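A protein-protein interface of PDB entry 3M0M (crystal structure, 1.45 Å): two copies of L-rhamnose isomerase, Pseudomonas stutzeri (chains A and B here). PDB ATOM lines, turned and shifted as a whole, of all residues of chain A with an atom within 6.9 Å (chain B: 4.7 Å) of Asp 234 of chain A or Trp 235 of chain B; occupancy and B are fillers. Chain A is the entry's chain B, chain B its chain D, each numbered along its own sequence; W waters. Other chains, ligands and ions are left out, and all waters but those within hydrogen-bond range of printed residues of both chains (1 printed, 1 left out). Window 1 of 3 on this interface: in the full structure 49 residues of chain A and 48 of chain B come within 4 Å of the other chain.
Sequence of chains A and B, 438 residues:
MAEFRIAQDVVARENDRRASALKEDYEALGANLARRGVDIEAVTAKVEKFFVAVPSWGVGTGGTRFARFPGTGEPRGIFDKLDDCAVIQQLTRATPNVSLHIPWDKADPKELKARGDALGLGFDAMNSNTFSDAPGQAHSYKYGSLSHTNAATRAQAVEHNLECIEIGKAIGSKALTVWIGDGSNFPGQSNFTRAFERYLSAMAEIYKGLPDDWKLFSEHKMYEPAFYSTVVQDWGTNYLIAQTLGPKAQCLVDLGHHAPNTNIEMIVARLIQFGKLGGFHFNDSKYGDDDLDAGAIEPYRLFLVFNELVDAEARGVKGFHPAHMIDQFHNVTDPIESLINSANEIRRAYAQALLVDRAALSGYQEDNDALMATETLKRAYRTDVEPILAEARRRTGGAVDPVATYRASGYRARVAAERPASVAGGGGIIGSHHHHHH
OD2 of Asp 234 of chain A lies within hydrogen-bond range of NE2 of Gln 233 of chain A (3.4 Å). OG1 of Thr 237 of chain A is in hydrogen-bond range of OE1 of Gln 233 of chain A. The backbone NH of Gly 236 of chain A lies within hydrogen-bond range of the side-chain carboxylate of Asp 234 of chain A (3.0 Å). The side-chain carboxylate of Asp 234 of chain A sits at hydrogen-bond distance from the backbone NH of Thr 237 of chain A (3.0 Å). OD1 of Asp 234 of chain B is in hydrogen-bond range of N of Gly 236 of chain B (3.0 Å). The side-chain carboxylate of Asp 234 of chain B is in hydrogen-bond range of the backbone NH of Thr 237 of chain B (3.1 Å).
Asp 234 of chain A touches Trp 235 of chain B, and with the chains exchanged Trp 235 of chain A touches Asp 234 of chain B. Trp 235 of chain A touches Gly 236 of chain B, and with the chains exchanged Gly 236 of chain A touches Trp 235 of chain B. Trp 235 of chain A touches Thr 237 of chain B, and with the chains exchanged Thr 237 of chain A touches Trp 235 of chain B. Positions printed for both chains: 220, 234, 235, 236, 237, 238, 239 and 267. Of the 10 pairs that touch across the chains among the printed residues, 6 have their exchanged pair printed and touching as well.
Water W1 lies within hydrogen-bond range of the side-chain carboxylate of Asp 234 of chain A and the side-chain carboxylate of Asp 234 of chain B.
Printed residues of chain A that touch a printed residue of chain B: Val 231, Asp 234, Trp 235, Gly 236, Thr 237 and Leu 240. Of the 10 printed residues of chain B, 6 touch a printed residue of chain A. Printed residues of chain B that touch a printed residue of chain A: Asp 234, Trp 235, Gly 236, Thr 237, Tyr 239 and Arg 270. Among the printed residues, 10 pairs touch across the chains. Among the printed residues, no Asp or Glu carboxylate lies within 4 Å of a Lys or Arg side-chain nitrogen of the other chain.
O of Val 231 of chain A is in hydrogen-bond range of NH2 of Arg 270 of chain B, 2.8 Å away. The side-chain carboxylate (OD2) of Asp 234 of chain A is in hydrogen-bond range of the indole nitrogen (NE1) of Trp 235 of chain B (2.7 Å). OD2 of Asp 234 of chain B is in hydrogen-bond range of NE1 of Trp 235 of chain A (2.8 Å). The guanidinium group of Arg 270 of chain B lies within hydrogen-bond range of the side-chain hydroxyl of Thr 237 of chain A (3.1 Å).
Trp 235 of chain A touches Gly 236 of chain B. Trp 235 of chain A touches Thr 237 of chain B. Gly 236 of chain A touches Trp 235 of chain B. Trp 235 of chain B touches Thr 237 of chain A (CZ2 to N, 3.5 Å). Trp 235 of chain B touches Leu 240 of chain A (CH2 to CD1, 3.8 Å). Leu 240 of chain A touches Tyr 239 of chain B (CD2 to CE2, 3.5 Å).
Asp 234 of chain A touches just one residue of chain B: Trp 235. Of chain A, only Asp 234 (2.7 Å), Gly 236 (3.7 Å), Thr 237 (3.5 Å) and Leu 240 (3.8 Å) come within 4 Å of Trp 235 of chain B. Printed residues of chain A within 4 Å of Arg 270 of chain B: Val 231 (2.8 Å) and Thr 237 (3.1 Å). Of the printed residues of chain B, Trp 235 of chain A touches Asp 234, Gly 236 and Thr 237. Of the printed residues of chain A, Gly 236 of chain B touches Trp 235 (3.7 Å). The nearest residue of chain A that does not touch Trp 235 of chain B is Gln 233 of chain A (4.2 Å).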
ATOM      1  N   GLU A 219     -17.637 -13.175  -3.311  1.00  0.00           N
ATOM      2  CA  GLU A 219     -17.951 -13.152  -4.735  1.00  0.00           C
ATOM      3  C   GLU A 219     -17.955 -14.542  -5.358  1.00  0.00           C
ATOM      4  O   GLU A 219     -16.913 -15.189  -5.436  1.00  0.00           O
ATOM      5  CB  GLU A 219     -16.925 -12.261  -5.448  1.00  0.00           C
ATOM      6  CG  GLU A 219     -17.082 -12.152  -6.957  1.00  0.00           C
ATOM      7  CD  GLU A 219     -16.078 -11.189  -7.574  1.00  0.00           C
ATOM      8  OE1 GLU A 219     -15.202 -10.678  -6.841  1.00  0.00           O
ATOM      9  OE2 GLU A 219     -16.159 -10.940  -8.797  1.00  0.00           O
ATOM     10  N   HIS A 220     -19.120 -14.999  -5.811  1.00  0.00           N
ATOM     11  CA  HIS A 220     -19.214 -16.318  -6.429  1.00  0.00           C
ATOM     12  C   HIS A 220     -18.741 -16.321  -7.879  1.00  0.00           C
ATOM     13  O   HIS A 220     -18.730 -15.288  -8.547  1.00  0.00           O
ATOM     14  CB  HIS A 220     -20.653 -16.855  -6.364  1.00  0.00           C
ATOM     15  CG  HIS A 220     -21.665 -15.993  -7.056  1.00  0.00           C
ATOM     16  ND1 HIS A 220     -22.392 -15.021  -6.400  1.00  0.00           N
ATOM     17  CD2 HIS A 220     -22.074 -15.960  -8.348  1.00  0.00           C
ATOM     18  CE1 HIS A 220     -23.205 -14.429  -7.257  1.00  0.00           C
ATOM     19  NE2 HIS A 220     -23.031 -14.979  -8.446  1.00  0.00           N
ATOM     20  N   LYS A 221     -18.337 -17.493  -8.356  1.00  0.00           N
ATOM     21  CA  LYS A 221     -17.880 -17.641  -9.732  1.00  0.00           C
ATOM     22  C   LYS A 221     -18.017 -19.108 -10.123  1.00  0.00           C
ATOM     23  O   LYS A 221     -17.549 -19.993  -9.407  1.00  0.00           O
ATOM     24  CB  LYS A 221     -16.427 -17.200  -9.874  1.00  0.00           C
ATOM     25  CG  LYS A 221     -16.022 -17.003 -11.325  1.00  0.00           C
ATOM     26  CD  LYS A 221     -14.569 -16.614 -11.462  1.00  0.00           C
ATOM     27  CE  LYS A 221     -14.223 -16.322 -12.915  1.00  0.00           C
ATOM     28  NZ  LYS A 221     -12.769 -16.040 -13.074  1.00  0.00           N
ATOM     29  N   MET A 222     -18.641 -19.366 -11.267  1.00  0.00           N
ATOM     30  CA  MET A 222     -18.865 -20.742 -11.693  1.00  0.00           C
ATOM     31  C   MET A 222     -17.594 -21.549 -11.924  1.00  0.00           C
ATOM     32  O   MET A 222     -17.517 -22.710 -11.527  1.00  0.00           O
ATOM     33  CB  MET A 222     -19.714 -20.758 -12.956  1.00  0.00           C
ATOM     34  CG  MET A 222     -20.080 -22.150 -13.436  1.00  0.00           C
ATOM     35  SD  MET A 222     -20.913 -22.048 -15.022  1.00  0.00           S
ATOM     36  CE  MET A 222     -21.874 -23.557 -15.029  1.00  0.00           C
ATOM     37  N   THR A 230     -15.839 -25.340  -7.968  1.00  0.00           N
ATOM     38  CA  THR A 230     -15.385 -24.117  -7.316  1.00  0.00           C
ATOM     39  C   THR A 230     -16.169 -24.040  -6.006  1.00  0.00           C
ATOM     40  O   THR A 230     -17.374 -24.266  -5.988  1.00  0.00           O
ATOM     41  CB  THR A 230     -15.661 -22.872  -8.196  1.00  0.00           C
ATOM     42  OG1 THR A 230     -14.806 -22.905  -9.347  1.00  0.00           O
ATOM     43  CG2 THR A 230     -15.380 -21.590  -7.422  1.00  0.00           C
ATOM     44  N   VAL A 231     -15.483 -23.742  -4.907  1.00  0.00           N
ATOM     45  CA  VAL A 231     -16.154 -23.677  -3.613  1.00  0.00           C
ATOM     46  C   VAL A 231     -17.311 -22.678  -3.599  1.00  0.00           C
ATOM     47  O   VAL A 231     -18.438 -23.032  -3.261  1.00  0.00           O
ATOM     48  CB  VAL A 231     -15.164 -23.332  -2.491  1.00  0.00           C
ATOM     49  CG1 VAL A 231     -15.895 -23.252  -1.156  1.00  0.00           C
ATOM     50  CG2 VAL A 231     -14.079 -24.398  -2.421  1.00  0.00           C
ATOM     51  N   VAL A 232     -17.036 -21.428  -3.950  1.00  0.00           N
ATOM     52  CA  VAL A 232     -18.093 -20.418  -3.990  1.00  0.00           C
ATOM     53  C   VAL A 232     -18.464 -20.337  -5.469  1.00  0.00           C
ATOM     54  O   VAL A 232     -18.077 -19.396  -6.168  1.00  0.00           O
ATOM     55  CB  VAL A 232     -17.576 -19.050  -3.500  1.00  0.00           C
ATOM     56  CG1 VAL A 232     -18.745 -18.096  -3.295  1.00  0.00           C
ATOM     57  CG2 VAL A 232     -16.785 -19.229  -2.205  1.00  0.00           C
ATOM     58  N   GLN A 233     -19.223 -21.328  -5.933  1.00  0.00           N
ATOM     59  CA  GLN A 233     -19.571 -21.431  -7.344  1.00  0.00           C
ATOM     60  C   GLN A 233     -20.762 -20.647  -7.868  1.00  0.00           C
ATOM     61  O   GLN A 233     -20.772 -20.279  -9.039  1.00  0.00           O
ATOM     62  CB  GLN A 233     -19.716 -22.915  -7.738  1.00  0.00           C
ATOM     63  CG  GLN A 233     -21.152 -23.449  -7.823  1.00  0.00           C
ATOM     64  CD  GLN A 233     -21.791 -23.681  -6.468  1.00  0.00           C
ATOM     65  OE1 GLN A 233     -21.446 -23.027  -5.483  1.00  0.00           O
ATOM     66  NE2 GLN A 233     -22.742 -24.598  -6.418  1.00  0.00           N
ATOM     67  N   ASP A 234     -21.767 -20.400  -7.034  1.00  0.00           N
ATOM     68  CA  ASP A 234     -22.924 -19.646  -7.505  1.00  0.00           C
ATOM     69  C   ASP A 234     -23.584 -18.851  -6.388  1.00  0.00           C
ATOM     70  O   ASP A 234     -23.128 -18.876  -5.244  1.00  0.00           O
ATOM     71  CB  ASP A 234     -23.942 -20.567  -8.201  1.00  0.00           C
ATOM     72  CG  ASP A 234     -24.530 -21.614  -7.279  1.00  0.00           C
ATOM     73  OD1 ASP A 234     -24.474 -21.444  -6.047  1.00  0.00           O
ATOM     74  OD2 ASP A 234     -25.076 -22.611  -7.798  1.00  0.00           O
ATOM     75  N   TRP A 235     -24.661 -18.147  -6.719  1.00  0.00           N
ATOM     76  CA  TRP A 235     -25.332 -17.316  -5.728  1.00  0.00           C
ATOM     77  C   TRP A 235     -25.997 -18.107  -4.607  1.00  0.00           C
ATOM     78  O   TRP A 235     -26.235 -17.563  -3.531  1.00  0.00           O
ATOM     79  CB  TRP A 235     -26.353 -16.393  -6.401  1.00  0.00           C
ATOM     80  CG  TRP A 235     -27.671 -17.025  -6.701  1.00  0.00           C
ATOM     81  CD1 TRP A 235     -27.978 -17.818  -7.767  1.00  0.00           C
ATOM     82  CD2 TRP A 235     -28.868 -16.918  -5.920  1.00  0.00           C
ATOM     83  NE1 TRP A 235     -29.293 -18.207  -7.705  1.00  0.00           N
ATOM     84  CE2 TRP A 235     -29.864 -17.670  -6.580  1.00  0.00           C
ATOM     85  CE3 TRP A 235     -29.196 -16.259  -4.729  1.00  0.00           C
ATOM     86  CZ2 TRP A 235     -31.168 -17.782  -6.090  1.00  0.00           C
ATOM     87  CZ3 TRP A 235     -30.501 -16.371  -4.238  1.00  0.00           C
ATOM     88  CH2 TRP A 235     -31.467 -17.128  -4.922  1.00  0.00           C
ATOM     89  N   GLY A 236     -26.297 -19.379  -4.859  1.00  0.00           N
ATOM     90  CA  GLY A 236     -26.911 -20.207  -3.834  1.00  0.00           C
ATOM     91  C   GLY A 236     -25.914 -20.431  -2.717  1.00  0.00           C
ATOM     92  O   GLY A 236     -26.222 -20.237  -1.539  1.00  0.00           O
ATOM     93  N   THR A 237     -24.710 -20.852  -3.082  1.00  0.00           N
ATOM     94  CA  THR A 237     -23.669 -21.065  -2.089  1.00  0.00           C
ATOM     95  C   THR A 237     -23.351 -19.718  -1.454  1.00  0.00           C
ATOM     96  O   THR A 237     -23.154 -19.619  -0.245  1.00  0.00           O
ATOM     97  CB  THR A 237     -22.401 -21.647  -2.732  1.00  0.00           C
ATOM     98  OG1 THR A 237     -22.665 -22.992  -3.140  1.00  0.00           O
ATOM     99  CG2 THR A 237     -21.235 -21.634  -1.752  1.00  0.00           C
ATOM    100  N   ASN A 238     -23.327 -18.671  -2.270  1.00  0.00           N
ATOM    101  CA  ASN A 238     -23.023 -17.345  -1.754  1.00  0.00           C
ATOM    102  C   ASN A 238     -24.041 -16.925  -0.696  1.00  0.00           C
ATOM    103  O   ASN A 238     -23.674 -16.362   0.332  1.00  0.00           O
ATOM    104  CB  ASN A 238     -22.984 -16.318  -2.890  1.00  0.00           C
ATOM    105  CG  ASN A 238     -21.983 -15.211  -2.626  1.00  0.00           C
ATOM    106  OD1 ASN A 238     -21.410 -15.133  -1.540  1.00  0.00           O
ATOM    107  ND2 ASN A 238     -21.760 -14.351  -3.618  1.00  0.00           N
ATOM    108  N   TYR A 239     -25.320 -17.200  -0.938  1.00  0.00           N
ATOM    109  CA  TYR A 239     -26.336 -16.840   0.043  1.00  0.00           C
ATOM    110  C   TYR A 239     -26.092 -17.596   1.343  1.00  0.00           C
ATOM    111  O   TYR A 239     -26.200 -17.026   2.426  1.00  0.00           O
ATOM    112  CB  TYR A 239     -27.741 -17.170  -0.457  1.00  0.00           C
ATOM    113  CG  TYR A 239     -28.789 -16.881   0.590  1.00  0.00           C
ATOM    114  CD1 TYR A 239     -29.215 -15.578   0.836  1.00  0.00           C
ATOM    115  CD2 TYR A 239     -29.304 -17.903   1.384  1.00  0.00           C
ATOM    116  CE1 TYR A 239     -30.122 -15.299   1.850  1.00  0.00           C
ATOM    117  CE2 TYR A 239     -30.208 -17.635   2.402  1.00  0.00           C
ATOM    118  CZ  TYR A 239     -30.612 -16.331   2.628  1.00  0.00           C
ATOM    119  OH  TYR A 239     -31.500 -16.065   3.644  1.00  0.00           O
ATOM    120  N   LEU A 240     -25.767 -18.880   1.234  1.00  0.00           N
ATOM    121  CA  LEU A 240     -25.510 -19.689   2.423  1.00  0.00           C
ATOM    122  C   LEU A 240     -24.365 -19.082   3.227  1.00  0.00           C
ATOM    123  O   LEU A 240     -24.403 -19.053   4.457  1.00  0.00           O
ATOM    124  CB  LEU A 240     -25.175 -21.131   2.025  1.00  0.00           C
ATOM    125  CG  LEU A 240     -26.324 -21.947   1.421  1.00  0.00           C
ATOM    126  CD1 LEU A 240     -25.804 -23.283   0.904  1.00  0.00           C
ATOM    127  CD2 LEU A 240     -27.401 -22.169   2.481  1.00  0.00           C
ATOM    128  N   ILE A 241     -23.346 -18.593   2.528  1.00  0.00           N
ATOM    129  CA  ILE A 241     -22.199 -17.969   3.184  1.00  0.00           C
ATOM    130  C   ILE A 241     -22.617 -16.713   3.944  1.00  0.00           C
ATOM    131  O   ILE A 241     -22.354 -16.577   5.145  1.00  0.00           O
ATOM    132  CB  ILE A 241     -21.113 -17.571   2.157  1.00  0.00           C
ATOM    133  CG1 ILE A 241     -20.535 -18.828   1.503  1.00  0.00           C
ATOM    134  CG2 ILE A 241     -20.013 -16.765   2.841  1.00  0.00           C
ATOM    135  CD1 ILE A 241     -19.671 -18.543   0.287  1.00  0.00           C
ATOM    136  N   HIS A 257     -19.830 -13.946 -14.117  1.00  0.00           N
ATOM    137  CA  HIS A 257     -19.544 -15.145 -13.328  1.00  0.00           C
ATOM    138  C   HIS A 257     -20.650 -16.197 -13.270  1.00  0.00           C
ATOM    139  O   HIS A 257     -20.682 -17.021 -12.347  1.00  0.00           O
ATOM    140  CB  HIS A 257     -19.186 -14.735 -11.895  1.00  0.00           C
ATOM    141  CG  HIS A 257     -17.853 -14.067 -11.763  1.00  0.00           C
ATOM    142  ND1 HIS A 257     -17.250 -13.855 -10.543  1.00  0.00           N
ATOM    143  CD2 HIS A 257     -16.995 -13.586 -12.695  1.00  0.00           C
ATOM    144  CE1 HIS A 257     -16.078 -13.275 -10.726  1.00  0.00           C
ATOM    145  NE2 HIS A 257     -15.898 -13.101 -12.022  1.00  0.00           N
ATOM    146  N   HIS A 258     -21.540 -16.195 -14.253  1.00  0.00           N
ATOM    147  CA  HIS A 258     -22.648 -17.136 -14.251  1.00  0.00           C
ATOM    148  C   HIS A 258     -22.664 -18.093 -15.433  1.00  0.00           C
ATOM    149  O   HIS A 258     -22.012 -17.860 -16.452  1.00  0.00           O
ATOM    150  CB  HIS A 258     -23.966 -16.355 -14.183  1.00  0.00           C
ATOM    151  CG  HIS A 258     -24.013 -15.374 -13.052  1.00  0.00           C
ATOM    152  ND1 HIS A 258     -23.458 -14.115 -13.133  1.00  0.00           N
ATOM    153  CD2 HIS A 258     -24.476 -15.501 -11.785  1.00  0.00           C
ATOM    154  CE1 HIS A 258     -23.575 -13.508 -11.964  1.00  0.00           C
ATOM    155  NE2 HIS A 258     -24.188 -14.329 -11.129  1.00  0.00           N
ATOM    156  N   ILE A 267     -31.400 -13.216 -10.057  1.00  0.00           N
ATOM    157  CA  ILE A 267     -30.515 -13.460  -8.920  1.00  0.00           C
ATOM    158  C   ILE A 267     -30.429 -12.175  -8.103  1.00  0.00           C
ATOM    159  O   ILE A 267     -30.503 -12.193  -6.878  1.00  0.00           O
ATOM    160  CB  ILE A 267     -29.105 -13.873  -9.393  1.00  0.00           C
ATOM    161  CG1 ILE A 267     -29.166 -15.281  -9.989  1.00  0.00           C
ATOM    162  CG2 ILE A 267     -28.104 -13.802  -8.233  1.00  0.00           C
ATOM    163  CD1 ILE A 267     -27.863 -15.740 -10.627  1.00  0.00           C
ATOM    164  N   HIS B 220     -37.093 -27.254  -8.640  1.00  0.00           N
ATOM    165  CA  HIS B 220     -36.651 -26.125  -9.448  1.00  0.00           C
ATOM    166  C   HIS B 220     -36.401 -26.509 -10.903  1.00  0.00           C
ATOM    167  O   HIS B 220     -36.177 -27.678 -11.228  1.00  0.00           O
ATOM    168  CB  HIS B 220     -35.381 -25.496  -8.856  1.00  0.00           C
ATOM    169  CG  HIS B 220     -34.213 -26.432  -8.775  1.00  0.00           C
ATOM    170  ND1 HIS B 220     -33.976 -27.242  -7.684  1.00  0.00           N
ATOM    171  CD2 HIS B 220     -33.215 -26.688  -9.654  1.00  0.00           C
ATOM    172  CE1 HIS B 220     -32.882 -27.953  -7.894  1.00  0.00           C
ATOM    173  NE2 HIS B 220     -32.401 -27.636  -9.082  1.00  0.00           N
ATOM    174  N   ASP B 234     -33.853 -22.140  -9.808  1.00  0.00           N
ATOM    175  CA  ASP B 234     -32.655 -22.907  -9.483  1.00  0.00           C
ATOM    176  C   ASP B 234     -32.630 -23.365  -8.032  1.00  0.00           C
ATOM    177  O   ASP B 234     -33.567 -23.104  -7.268  1.00  0.00           O
ATOM    178  CB  ASP B 234     -31.378 -22.119  -9.828  1.00  0.00           C
ATOM    179  CG  ASP B 234     -31.232 -20.836  -9.036  1.00  0.00           C
ATOM    180  OD1 ASP B 234     -31.809 -20.727  -7.941  1.00  0.00           O
ATOM    181  OD2 ASP B 234     -30.510 -19.935  -9.506  1.00  0.00           O
ATOM    182  N   TRP B 235     -31.556 -24.046  -7.648  1.00  0.00           N
ATOM    183  CA  TRP B 235     -31.468 -24.578  -6.297  1.00  0.00           C
ATOM    184  C   TRP B 235     -31.359 -23.525  -5.200  1.00  0.00           C
ATOM    185  O   TRP B 235     -31.674 -23.810  -4.047  1.00  0.00           O
ATOM    186  CB  TRP B 235     -30.314 -25.577  -6.186  1.00  0.00           C
ATOM    187  CG  TRP B 235     -28.971 -24.959  -6.001  1.00  0.00           C
ATOM    188  CD1 TRP B 235     -28.164 -24.428  -6.966  1.00  0.00           C
ATOM    189  CD2 TRP B 235     -28.274 -24.802  -4.762  1.00  0.00           C
ATOM    190  NE1 TRP B 235     -27.003 -23.951  -6.400  1.00  0.00           N
ATOM    191  CE2 TRP B 235     -27.048 -24.169  -5.048  1.00  0.00           C
ATOM    192  CE3 TRP B 235     -28.571 -25.138  -3.433  1.00  0.00           C
ATOM    193  CZ2 TRP B 235     -26.113 -23.862  -4.054  1.00  0.00           C
ATOM    194  CZ3 TRP B 235     -27.639 -24.832  -2.443  1.00  0.00           C
ATOM    195  CH2 TRP B 235     -26.426 -24.202  -2.761  1.00  0.00           C
ATOM    196  N   GLY B 236     -30.923 -22.316  -5.555  1.00  0.00           N
ATOM    197  CA  GLY B 236     -30.815 -21.249  -4.571  1.00  0.00           C
ATOM    198  C   GLY B 236     -32.205 -20.815  -4.150  1.00  0.00           C
ATOM    199  O   GLY B 236     -32.511 -20.730  -2.962  1.00  0.00           O
ATOM    200  N   THR B 237     -33.059 -20.542  -5.129  1.00  0.00           N
ATOM    201  CA  THR B 237     -34.429 -20.158  -4.833  1.00  0.00           C
ATOM    202  C   THR B 237     -35.099 -21.332  -4.124  1.00  0.00           C
ATOM    203  O   THR B 237     -35.870 -21.148  -3.180  1.00  0.00           O
ATOM    204  CB  THR B 237     -35.200 -19.825  -6.124  1.00  0.00           C
ATOM    205  OG1 THR B 237     -34.685 -18.606  -6.678  1.00  0.00           O
ATOM    206  CG2 THR B 237     -36.691 -19.658  -5.844  1.00  0.00           C
ATOM    207  N   ASN B 238     -34.785 -22.547  -4.567  1.00  0.00           N
ATOM    208  CA  ASN B 238     -35.380 -23.728  -3.958  1.00  0.00           C
ATOM    209  C   ASN B 238     -34.999 -23.815  -2.479  1.00  0.00           C
ATOM    210  O   ASN B 238     -35.846 -24.114  -1.627  1.00  0.00           O
ATOM    211  CB  ASN B 238     -34.949 -24.997  -4.699  1.00  0.00           C
ATOM    212  CG  ASN B 238     -36.017 -26.068  -4.667  1.00  0.00           C
ATOM    213  OD1 ASN B 238     -37.033 -25.922  -3.983  1.00  0.00           O
ATOM    214  ND2 ASN B 238     -35.804 -27.150  -5.408  1.00  0.00           N
ATOM    215  N   TYR B 239     -33.736 -23.541  -2.162  1.00  0.00           N
ATOM    216  CA  TYR B 239     -33.320 -23.587  -0.764  1.00  0.00           C
ATOM    217  C   TYR B 239     -34.103 -22.566   0.061  1.00  0.00           C
ATOM    218  O   TYR B 239     -34.537 -22.857   1.175  1.00  0.00           O
ATOM    219  CB  TYR B 239     -31.826 -23.303  -0.618  1.00  0.00           C
ATOM    220  CG  TYR B 239     -31.405 -23.241   0.830  1.00  0.00           C
ATOM    221  CD1 TYR B 239     -31.290 -24.403   1.594  1.00  0.00           C
ATOM    222  CD2 TYR B 239     -31.193 -22.015   1.456  1.00  0.00           C
ATOM    223  CE1 TYR B 239     -30.976 -24.341   2.950  1.00  0.00           C
ATOM    224  CE2 TYR B 239     -30.882 -21.941   2.811  1.00  0.00           C
ATOM    225  CZ  TYR B 239     -30.776 -23.107   3.549  1.00  0.00           C
ATOM    226  OH  TYR B 239     -30.473 -23.031   4.890  1.00  0.00           O
ATOM    227  N   ILE B 267     -24.367 -29.258  -6.172  1.00  0.00           N
ATOM    228  CA  ILE B 267     -25.657 -28.802  -5.655  1.00  0.00           C
ATOM    229  C   ILE B 267     -26.181 -29.858  -4.690  1.00  0.00           C
ATOM    230  O   ILE B 267     -26.692 -29.539  -3.614  1.00  0.00           O
ATOM    231  CB  ILE B 267     -26.675 -28.595  -6.798  1.00  0.00           C
ATOM    232  CG1 ILE B 267     -26.257 -27.385  -7.637  1.00  0.00           C
ATOM    233  CG2 ILE B 267     -28.087 -28.414  -6.232  1.00  0.00           C
ATOM    234  CD1 ILE B 267     -27.090 -27.192  -8.889  1.00  0.00           C
ATOM    235  N   ARG B 270     -24.335 -29.570  -1.430  1.00  0.00           N
ATOM    236  CA  ARG B 270     -24.750 -28.395  -0.669  1.00  0.00           C
ATOM    237  C   ARG B 270     -26.090 -28.608   0.025  1.00  0.00           C
ATOM    238  O   ARG B 270     -26.247 -28.279   1.205  1.00  0.00           O
ATOM    239  CB  ARG B 270     -24.831 -27.172  -1.587  1.00  0.00           C
ATOM    240  CG  ARG B 270     -23.486 -26.704  -2.138  1.00  0.00           C
ATOM    241  CD  ARG B 270     -22.691 -25.905  -1.101  1.00  0.00           C
ATOM    242  NE  ARG B 270     -21.443 -25.371  -1.644  1.00  0.00           N
ATOM    243  CZ  ARG B 270     -20.280 -26.017  -1.641  1.00  0.00           C
ATOM    244  NH1 ARG B 270     -20.188 -27.236  -1.122  1.00  0.00           N
ATOM    245  NH2 ARG B 270     -19.205 -25.441  -2.162  1.00  0.00           N
ATOM    246  N   LEU B 271     -27.060 -29.156  -0.697  1.00  0.00           N
ATOM    247  CA  LEU B 271     -28.373 -29.395  -0.110  1.00  0.00           C
ATOM    248  C   LEU B 271     -28.304 -30.398   1.039  1.00  0.00           C
ATOM    249  O   LEU B 271     -29.025 -30.266   2.026  1.00  0.00           O
ATOM    250  CB  LEU B 271     -29.351 -29.869  -1.188  1.00  0.00           C
ATOM    251  CG  LEU B 271     -29.797 -28.745  -2.130  1.00  0.00           C
ATOM    252  CD1 LEU B 271     -30.562 -29.323  -3.307  1.00  0.00           C
ATOM    253  CD2 LEU B 271     -30.659 -27.746  -1.364  1.00  0.00           C
HETATM  254  O   HOH W   1     -27.530 -21.346  -9.468  1.00  0.00           O
